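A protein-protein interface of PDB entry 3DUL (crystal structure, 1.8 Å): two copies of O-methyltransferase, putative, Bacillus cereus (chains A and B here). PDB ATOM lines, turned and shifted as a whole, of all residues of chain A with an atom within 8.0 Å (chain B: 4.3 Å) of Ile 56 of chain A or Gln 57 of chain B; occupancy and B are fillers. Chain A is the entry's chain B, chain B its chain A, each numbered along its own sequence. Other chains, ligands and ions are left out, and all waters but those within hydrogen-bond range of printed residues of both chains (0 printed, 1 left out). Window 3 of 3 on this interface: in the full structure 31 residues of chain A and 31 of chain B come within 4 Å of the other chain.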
ATOM      1  N   PHE A  49      29.291  -9.568  15.240  1.00  0.00           N
ATOM      2  CA  PHE A  49      28.153 -10.112  14.502  1.00  0.00           C
ATOM      3  C   PHE A  49      28.038 -11.600  14.788  1.00  0.00           C
ATOM      4  O   PHE A  49      26.953 -12.128  15.043  1.00  0.00           O
ATOM      5  CB  PHE A  49      28.352  -9.900  13.001  1.00  0.00           C
ATOM      6  CG  PHE A  49      27.324 -10.589  12.151  1.00  0.00           C
ATOM      7  CD1 PHE A  49      26.086 -10.002  11.914  1.00  0.00           C
ATOM      8  CD2 PHE A  49      27.593 -11.834  11.592  1.00  0.00           C
ATOM      9  CE1 PHE A  49      25.128 -10.647  11.128  1.00  0.00           C
ATOM     10  CE2 PHE A  49      26.642 -12.486  10.807  1.00  0.00           C
ATOM     11  CZ  PHE A  49      25.407 -11.886  10.575  1.00  0.00           C
ATOM     12  N   LEU A  50      29.169 -12.292  14.736  1.00  0.00           N
ATOM     13  CA  LEU A  50      29.156 -13.716  15.003  1.00  0.00           C
ATOM     14  C   LEU A  50      28.706 -14.011  16.432  1.00  0.00           C
ATOM     15  O   LEU A  50      27.854 -14.872  16.652  1.00  0.00           O
ATOM     16  CB  LEU A  50      30.545 -14.312  14.753  1.00  0.00           C
ATOM     17  CG  LEU A  50      31.014 -14.295  13.290  1.00  0.00           C
ATOM     18  CD1 LEU A  50      32.461 -14.764  13.222  1.00  0.00           C
ATOM     19  CD2 LEU A  50      30.118 -15.189  12.437  1.00  0.00           C
ATOM     20  N   GLN A  51      29.276 -13.312  17.409  1.00  0.00           N
ATOM     21  CA  GLN A  51      28.891 -13.565  18.795  1.00  0.00           C
ATOM     22  C   GLN A  51      27.386 -13.308  18.996  1.00  0.00           C
ATOM     23  O   GLN A  51      26.673 -14.163  19.520  1.00  0.00           O
ATOM     24  CB  GLN A  51      29.695 -12.691  19.761  1.00  0.00           C
ATOM     25  CG  GLN A  51      29.444 -13.065  21.217  1.00  0.00           C
ATOM     26  CD  GLN A  51      29.987 -12.044  22.204  1.00  0.00           C
ATOM     27  OE1 GLN A  51      29.896 -12.234  23.420  1.00  0.00           O
ATOM     28  NE2 GLN A  51      30.540 -10.959  21.691  1.00  0.00           N
ATOM     29  N   LEU A  52      26.917 -12.145  18.557  1.00  0.00           N
ATOM     30  CA  LEU A  52      25.504 -11.781  18.689  1.00  0.00           C
ATOM     31  C   LEU A  52      24.585 -12.791  18.000  1.00  0.00           C
ATOM     32  O   LEU A  52      23.588 -13.224  18.580  1.00  0.00           O
ATOM     33  CB  LEU A  52      25.254 -10.387  18.105  1.00  0.00           C
ATOM     34  CG  LEU A  52      25.923  -9.199  18.811  1.00  0.00           C
ATOM     35  CD1 LEU A  52      25.657  -7.921  18.035  1.00  0.00           C
ATOM     36  CD2 LEU A  52      25.398  -9.082  20.235  1.00  0.00           C
ATOM     37  N   LEU A  53      24.917 -13.178  16.770  1.00  0.00           N
ATOM     38  CA  LEU A  53      24.076 -14.130  16.051  1.00  0.00           C
ATOM     39  C   LEU A  53      24.032 -15.471  16.769  1.00  0.00           C
ATOM     40  O   LEU A  53      22.989 -16.123  16.821  1.00  0.00           O
ATOM     41  CB  LEU A  53      24.563 -14.318  14.612  1.00  0.00           C
ATOM     42  CG  LEU A  53      23.519 -14.977  13.700  1.00  0.00           C
ATOM     43  CD1 LEU A  53      22.218 -14.183  13.776  1.00  0.00           C
ATOM     44  CD2 LEU A  53      24.028 -15.023  12.256  1.00  0.00           C
ATOM     45  N   VAL A  54      25.163 -15.891  17.333  1.00  0.00           N
ATOM     46  CA  VAL A  54      25.205 -17.147  18.070  1.00  0.00           C
ATOM     47  C   VAL A  54      24.257 -17.010  19.270  1.00  0.00           C
ATOM     48  O   VAL A  54      23.514 -17.933  19.605  1.00  0.00           O
ATOM     49  CB  VAL A  54      26.644 -17.459  18.580  1.00  0.00           C
ATOM     50  CG1 VAL A  54      26.605 -18.484  19.697  1.00  0.00           C
ATOM     51  CG2 VAL A  54      27.497 -17.995  17.425  1.00  0.00           C
ATOM     52  N   GLN A  55      24.274 -15.839  19.893  1.00  0.00           N
ATOM     53  CA  GLN A  55      23.430 -15.586  21.057  1.00  0.00           C
ATOM     54  C   GLN A  55      21.952 -15.530  20.675  1.00  0.00           C
ATOM     55  O   GLN A  55      21.103 -16.090  21.367  1.00  0.00           O
ATOM     56  CB  GLN A  55      23.859 -14.278  21.738  1.00  0.00           C
ATOM     57  CG  GLN A  55      25.331 -14.286  22.143  1.00  0.00           C
ATOM     58  CD  GLN A  55      25.738 -13.121  23.028  1.00  0.00           C
ATOM     59  OE1 GLN A  55      25.340 -11.980  22.799  1.00  0.00           O
ATOM     60  NE2 GLN A  55      26.558 -13.405  24.035  1.00  0.00           N
ATOM     61  N   ILE A  56      21.652 -14.870  19.567  1.00  0.00           N
ATOM     62  CA  ILE A  56      20.266 -14.761  19.111  1.00  0.00           C
ATOM     63  C   ILE A  56      19.723 -16.145  18.813  1.00  0.00           C
ATOM     64  O   ILE A  56      18.627 -16.498  19.251  1.00  0.00           O
ATOM     65  CB  ILE A  56      20.167 -13.869  17.869  1.00  0.00           C
ATOM     66  CG1 ILE A  56      20.520 -12.438  18.254  1.00  0.00           C
ATOM     67  CG2 ILE A  56      18.748 -13.932  17.270  1.00  0.00           C
ATOM     68  CD1 ILE A  56      20.639 -11.508  17.096  1.00  0.00           C
ATOM     69  N   GLN A  57      20.492 -16.950  18.085  1.00  0.00           N
ATOM     70  CA  GLN A  57      20.037 -18.298  17.792  1.00  0.00           C
ATOM     71  C   GLN A  57      20.060 -19.200  19.021  1.00  0.00           C
ATOM     72  O   GLN A  57      19.263 -20.130  19.125  1.00  0.00           O
ATOM     73  CB  GLN A  57      20.888 -18.960  16.700  1.00  0.00           C
ATOM     74  CG  GLN A  57      20.417 -20.387  16.418  1.00  0.00           C
ATOM     75  CD  GLN A  57      21.350 -21.164  15.533  1.00  0.00           C
ATOM     76  OE1 GLN A  57      22.569 -20.997  15.604  1.00  0.00           O
ATOM     77  NE2 GLN A  57      20.790 -22.041  14.703  1.00  0.00           N
ATOM     78  N   GLY A  58      20.961 -18.923  19.959  1.00  0.00           N
ATOM     79  CA  GLY A  58      21.073 -19.768  21.135  1.00  0.00           C
ATOM     80  C   GLY A  58      21.841 -21.028  20.756  1.00  0.00           C
ATOM     81  O   GLY A  58      21.578 -22.118  21.263  1.00  0.00           O
ATOM     82  N   ALA A  59      22.797 -20.874  19.844  1.00  0.00           N
ATOM     83  CA  ALA A  59      23.609 -21.999  19.375  1.00  0.00           C
ATOM     84  C   ALA A  59      24.378 -22.677  20.508  1.00  0.00           C
ATOM     85  O   ALA A  59      24.881 -22.007  21.404  1.00  0.00           O
ATOM     86  CB  ALA A  59      24.579 -21.503  18.305  1.00  0.00           C
ATOM     87  N   GLY A  79      29.928 -16.458  22.451  1.00  0.00           N
ATOM     88  CA  GLY A  79      28.488 -16.445  22.269  1.00  0.00           C
ATOM     89  C   GLY A  79      27.760 -17.631  22.878  1.00  0.00           C
ATOM     90  O   GLY A  79      26.538 -17.612  22.996  1.00  0.00           O
ATOM     91  N   PHE A 136      25.288 -23.981  14.308  1.00  0.00           N
ATOM     92  CA  PHE A 136      25.855 -22.788  13.693  1.00  0.00           C
ATOM     93  C   PHE A 136      27.195 -23.174  13.066  1.00  0.00           C
ATOM     94  O   PHE A 136      27.972 -23.904  13.679  1.00  0.00           O
ATOM     95  CB  PHE A 136      26.062 -21.738  14.796  1.00  0.00           C
ATOM     96  CG  PHE A 136      26.323 -20.347  14.301  1.00  0.00           C
ATOM     97  CD1 PHE A 136      27.556 -19.993  13.772  1.00  0.00           C
ATOM     98  CD2 PHE A 136      25.334 -19.366  14.410  1.00  0.00           C
ATOM     99  CE1 PHE A 136      27.809 -18.698  13.362  1.00  0.00           C
ATOM    100  CE2 PHE A 136      25.577 -18.062  14.003  1.00  0.00           C
ATOM    101  CZ  PHE A 136      26.818 -17.723  13.476  1.00  0.00           C
ATOM    102  N   VAL A 162      22.369 -22.262  11.101  1.00  0.00           N
ATOM    103  CA  VAL A 162      22.791 -21.014  10.495  1.00  0.00           C
ATOM    104  C   VAL A 162      24.191 -21.269   9.962  1.00  0.00           C
ATOM    105  O   VAL A 162      25.004 -21.886  10.648  1.00  0.00           O
ATOM    106  CB  VAL A 162      22.856 -19.875  11.537  1.00  0.00           C
ATOM    107  CG1 VAL A 162      23.436 -18.615  10.916  1.00  0.00           C
ATOM    108  CG2 VAL A 162      21.443 -19.591  12.076  1.00  0.00           C
ATOM    109  N   LEU B  53      16.570 -13.237  10.016  1.00  0.00           N
ATOM    110  CA  LEU B  53      16.880 -12.898  11.407  1.00  0.00           C
ATOM    111  C   LEU B  53      15.666 -13.125  12.293  1.00  0.00           C
ATOM    112  O   LEU B  53      15.770 -13.657  13.396  1.00  0.00           O
ATOM    113  CB  LEU B  53      17.325 -11.446  11.515  1.00  0.00           C
ATOM    114  CG  LEU B  53      18.498 -11.196  12.461  1.00  0.00           C
ATOM    115  CD1 LEU B  53      18.628  -9.710  12.686  1.00  0.00           C
ATOM    116  CD2 LEU B  53      18.303 -11.920  13.768  1.00  0.00           C
ATOM    117  N   VAL B  54      14.510 -12.715  11.792  1.00  0.00           N
ATOM    118  CA  VAL B  54      13.264 -12.905  12.527  1.00  0.00           C
ATOM    119  C   VAL B  54      13.079 -14.406  12.742  1.00  0.00           C
ATOM    120  O   VAL B  54      12.727 -14.856  13.832  1.00  0.00           O
ATOM    121  CB  VAL B  54      12.068 -12.312  11.725  1.00  0.00           C
ATOM    122  CG1 VAL B  54      10.743 -12.835  12.269  1.00  0.00           C
ATOM    123  CG2 VAL B  54      12.107 -10.791  11.787  1.00  0.00           C
ATOM    124  N   GLN B  55      13.348 -15.193  11.706  1.00  0.00           N
ATOM    125  CA  GLN B  55      13.194 -16.628  11.813  1.00  0.00           C
ATOM    126  C   GLN B  55      14.216 -17.240  12.773  1.00  0.00           C
ATOM    127  O   GLN B  55      13.890 -18.127  13.545  1.00  0.00           O
ATOM    128  CB  GLN B  55      13.298 -17.265  10.424  1.00  0.00           C
ATOM    129  CG  GLN B  55      12.294 -16.668   9.443  1.00  0.00           C
ATOM    130  CD  GLN B  55      12.217 -17.409   8.124  1.00  0.00           C
ATOM    131  OE1 GLN B  55      13.238 -17.774   7.540  1.00  0.00           O
ATOM    132  NE2 GLN B  55      11.000 -17.616   7.635  1.00  0.00           N
ATOM    133  N   ILE B  56      15.451 -16.757  12.732  1.00  0.00           N
ATOM    134  CA  ILE B  56      16.472 -17.297  13.631  1.00  0.00           C
ATOM    135  C   ILE B  56      16.112 -17.009  15.074  1.00  0.00           C
ATOM    136  O   ILE B  56      16.210 -17.879  15.933  1.00  0.00           O
ATOM    137  CB  ILE B  56      17.851 -16.697  13.331  1.00  0.00           C
ATOM    138  CG1 ILE B  56      18.314 -17.182  11.956  1.00  0.00           C
ATOM    139  CG2 ILE B  56      18.861 -17.110  14.422  1.00  0.00           C
ATOM    140  CD1 ILE B  56      19.467 -16.390  11.382  1.00  0.00           C
ATOM    141  N   GLN B  57      15.681 -15.785  15.342  1.00  0.00           N
ATOM    142  CA  GLN B  57      15.315 -15.443  16.702  1.00  0.00           C
ATOM    143  C   GLN B  57      14.016 -16.148  17.066  1.00  0.00           C
ATOM    144  O   GLN B  57      13.846 -16.609  18.192  1.00  0.00           O
ATOM    145  CB  GLN B  57      15.129 -13.933  16.864  1.00  0.00           C
ATOM    146  CG  GLN B  57      14.789 -13.550  18.306  1.00  0.00           C
ATOM    147  CD  GLN B  57      14.438 -12.095  18.468  1.00  0.00           C
ATOM    148  OE1 GLN B  57      13.957 -11.456  17.532  1.00  0.00           O
ATOM    149  NE2 GLN B  57      14.653 -11.561  19.668  1.00  0.00           N
ATOM    150  N   GLY B  58      13.112 -16.249  16.096  1.00  0.00           N
ATOM    151  CA  GLY B  58      11.822 -16.870  16.353  1.00  0.00           C
ATOM    152  C   GLY B  58      10.912 -15.790  16.916  1.00  0.00           C
ATOM    153  O   GLY B  58      10.086 -16.047  17.795  1.00  0.00           O
ATOM    154  N   ALA B  59      11.073 -14.575  16.401  1.00  0.00           N
ATOM    155  CA  ALA B  59      10.296 -13.413  16.850  1.00  0.00           C
ATOM    156  C   ALA B  59       8.800 -13.574  16.606  1.00  0.00           C
ATOM    157  O   ALA B  59       8.387 -14.081  15.564  1.00  0.00           O
ATOM    158  CB  ALA B  59      10.795 -12.171  16.153  1.00  0.00           C
ATOM    159  N   ASP B 135       9.902  -8.384  20.566  1.00  0.00           N
ATOM    160  CA  ASP B 135      11.070  -9.276  20.472  1.00  0.00           C
ATOM    161  C   ASP B 135      12.036  -8.785  19.396  1.00  0.00           C
ATOM    162  O   ASP B 135      13.234  -9.092  19.433  1.00  0.00           O
ATOM    163  CB  ASP B 135      10.686 -10.699  20.040  1.00  0.00           C
ATOM    164  CG  ASP B 135       9.558 -11.296  20.841  1.00  0.00           C
ATOM    165  OD1 ASP B 135       9.596 -11.244  22.089  1.00  0.00           O
ATOM    166  OD2 ASP B 135       8.636 -11.855  20.204  1.00  0.00           O
ATOM    167  N   PHE B 136      11.508  -8.048  18.425  1.00  0.00           N
ATOM    168  CA  PHE B 136      12.305  -7.577  17.300  1.00  0.00           C
ATOM    169  C   PHE B 136      11.787  -6.207  16.861  1.00  0.00           C
ATOM    170  O   PHE B 136      10.577  -6.002  16.740  1.00  0.00           O
ATOM    171  CB  PHE B 136      12.166  -8.609  16.168  1.00  0.00           C
ATOM    172  CG  PHE B 136      13.169  -8.468  15.058  1.00  0.00           C
ATOM    173  CD1 PHE B 136      13.089  -7.424  14.148  1.00  0.00           C
ATOM    174  CD2 PHE B 136      14.171  -9.425  14.897  1.00  0.00           C
ATOM    175  CE1 PHE B 136      13.982  -7.326  13.092  1.00  0.00           C
ATOM    176  CE2 PHE B 136      15.075  -9.336  13.834  1.00  0.00           C
ATOM    177  CZ  PHE B 136      14.979  -8.286  12.934  1.00  0.00           C
ATOM    178  N   GLY B 160      17.121  -9.558  25.336  1.00  0.00           N
ATOM    179  CA  GLY B 160      17.119 -10.477  24.214  1.00  0.00           C
ATOM    180  C   GLY B 160      16.519  -9.861  22.961  1.00  0.00           C
ATOM    181  O   GLY B 160      16.658 -10.405  21.864  1.00  0.00           O
ATOM    182  N   THR B 161      15.829  -8.730  23.110  1.00  0.00           N
ATOM    183  CA  THR B 161      15.234  -8.071  21.951  1.00  0.00           C
ATOM    184  C   THR B 161      16.273  -7.666  20.924  1.00  0.00           C
ATOM    185  O   THR B 161      17.313  -7.124  21.274  1.00  0.00           O
ATOM    186  CB  THR B 161      14.481  -6.797  22.355  1.00  0.00           C
ATOM    187  OG1 THR B 161      13.311  -7.166  23.086  1.00  0.00           O
ATOM    188  CG2 THR B 161      14.102  -5.985  21.134  1.00  0.00           C
ATOM    189  N   VAL B 162      15.977  -7.936  19.657  1.00  0.00           N
ATOM    190  CA  VAL B 162      16.864  -7.555  18.574  1.00  0.00           C
ATOM    191  C   VAL B 162      16.382  -6.229  18.000  1.00  0.00           C
ATOM    192  O   VAL B 162      15.183  -6.049  17.752  1.00  0.00           O
ATOM    193  CB  VAL B 162      16.868  -8.620  17.448  1.00  0.00           C
ATOM    194  CG1 VAL B 162      17.697  -8.137  16.264  1.00  0.00           C
ATOM    195  CG2 VAL B 162      17.410  -9.927  17.991  1.00  0.00           C
ATOM    196  N   MET B 218      23.056  -3.453  14.230  1.00  0.00           N
ATOM    197  CA  MET B 218      22.337  -4.625  14.698  1.00  0.00           C
ATOM    198  C   MET B 218      22.673  -4.685  16.175  1.00  0.00           C
ATOM    199  O   MET B 218      23.842  -4.804  16.549  1.00  0.00           O
ATOM    200  CB  MET B 218      22.808  -5.903  14.000  1.00  0.00           C
ATOM    201  CG  MET B 218      22.239  -7.162  14.642  1.00  0.00           C
ATOM    202  SD  MET B 218      22.728  -8.825  13.771  1.00  0.00           S
ATOM    203  CE  MET B 218      21.321  -9.933  14.438  1.00  0.00           C
ATOM    204  N   VAL B 220      21.463  -6.057  20.335  1.00  0.00           N
ATOM    205  CA  VAL B 220      20.692  -6.972  21.167  1.00  0.00           C
ATOM    206  C   VAL B 220      20.636  -6.381  22.573  1.00  0.00           C
ATOM    207  O   VAL B 220      21.658  -5.979  23.131  1.00  0.00           O
ATOM    208  CB  VAL B 220      21.325  -8.378  21.231  1.00  0.00           C
ATOM    209  CG1 VAL B 220      20.505  -9.268  22.147  1.00  0.00           C
ATOM    210  CG2 VAL B 220      21.376  -8.988  19.837  1.00  0.00           C
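The side-chain amide nitrogen (NE2) of Gln 57 of chain B lies within hydrogen-bond range of the backbone carbonyl oxygen (O) of Asp 135 of chain B, 2.9 Å away.
The side-chain amide nitrogen (NE2) of Gln 57 of chain B sits at hydrogen-bond distance from the backbone carbonyl oxygen (O) of Gly 160 of chain B (3.2 Å).
N of Val 162 of chain B is in hydrogen-bond range of O of Asp 135 of chain B.
Among the printed residues, merely in contact across the chains: Leu 52 of chain A with Met 218 of chain B (3.9 Å), Ile 56 of chain A with Gln 57 of chain B (3.6 Å), Ile 56 of chain A with Val 162 of chain B (3.7 Å), Ile 56 of chain A with Met 218 of chain B (3.2 Å), Ile 56 of chain A with Val 220 of chain B (3.8 Å), Gln 57 of chain A with Ile 56 of chain B (3.6 Å) and Val 162 of chain A with Ile 56 of chain B (3.8 Å).
Printed residues of chain B within 4 Å of Leu 52 of chain A: Met 218 (3.9 Å).
Of chain B, only Gln 57 (3.6 Å), Val 162 (3.7 Å), Met 218 (3.2 Å) and Val 220 (3.8 Å) come within 4 Å of Ile 56 of chain A.
Of the printed residues of chain B, Gln 57 of chain A touches Ile 56.
Gly 79 of chain A touches none of the printed residues of chain B.
Of the printed residues of chain A, Ile 56 of chain B touches Gln 57 and Val 162.
Of chain A, only Ile 56 (3.6 Å) comes within 4 Å of Gln 57 of chain B.
No residue of chain A comes within 4 Å of Gly 58 of chain B.
Of the printed residues of chain A, Met 218 of chain B touches Leu 52 and Ile 56.
The nearest residue of chain A that does not touch Gln 57 of chain B is Gln 57 of chain A (5.6 Å).
Printed residues of chain B that touch a printed residue of chain A: Ile 56, Gln 57, Val 162, Met 218 and Val 220.
Among the printed residues, no Asp or Glu carboxylate lies within 4 Å of a Lys or Arg side-chain nitrogen of the other chain.
Ile 56 of chain A touches Gln 57 of chain B, and with the chains exchanged Gln 57 of chain A touches Ile 56 of chain B.
Ile 56 of chain A touches Val 162 of chain B, and with the chains exchanged Val 162 of chain A touches Ile 56 of chain B.
Positions printed for both chains: 53, 54, 55, 56, 57, 58, 59, 136 and 162.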
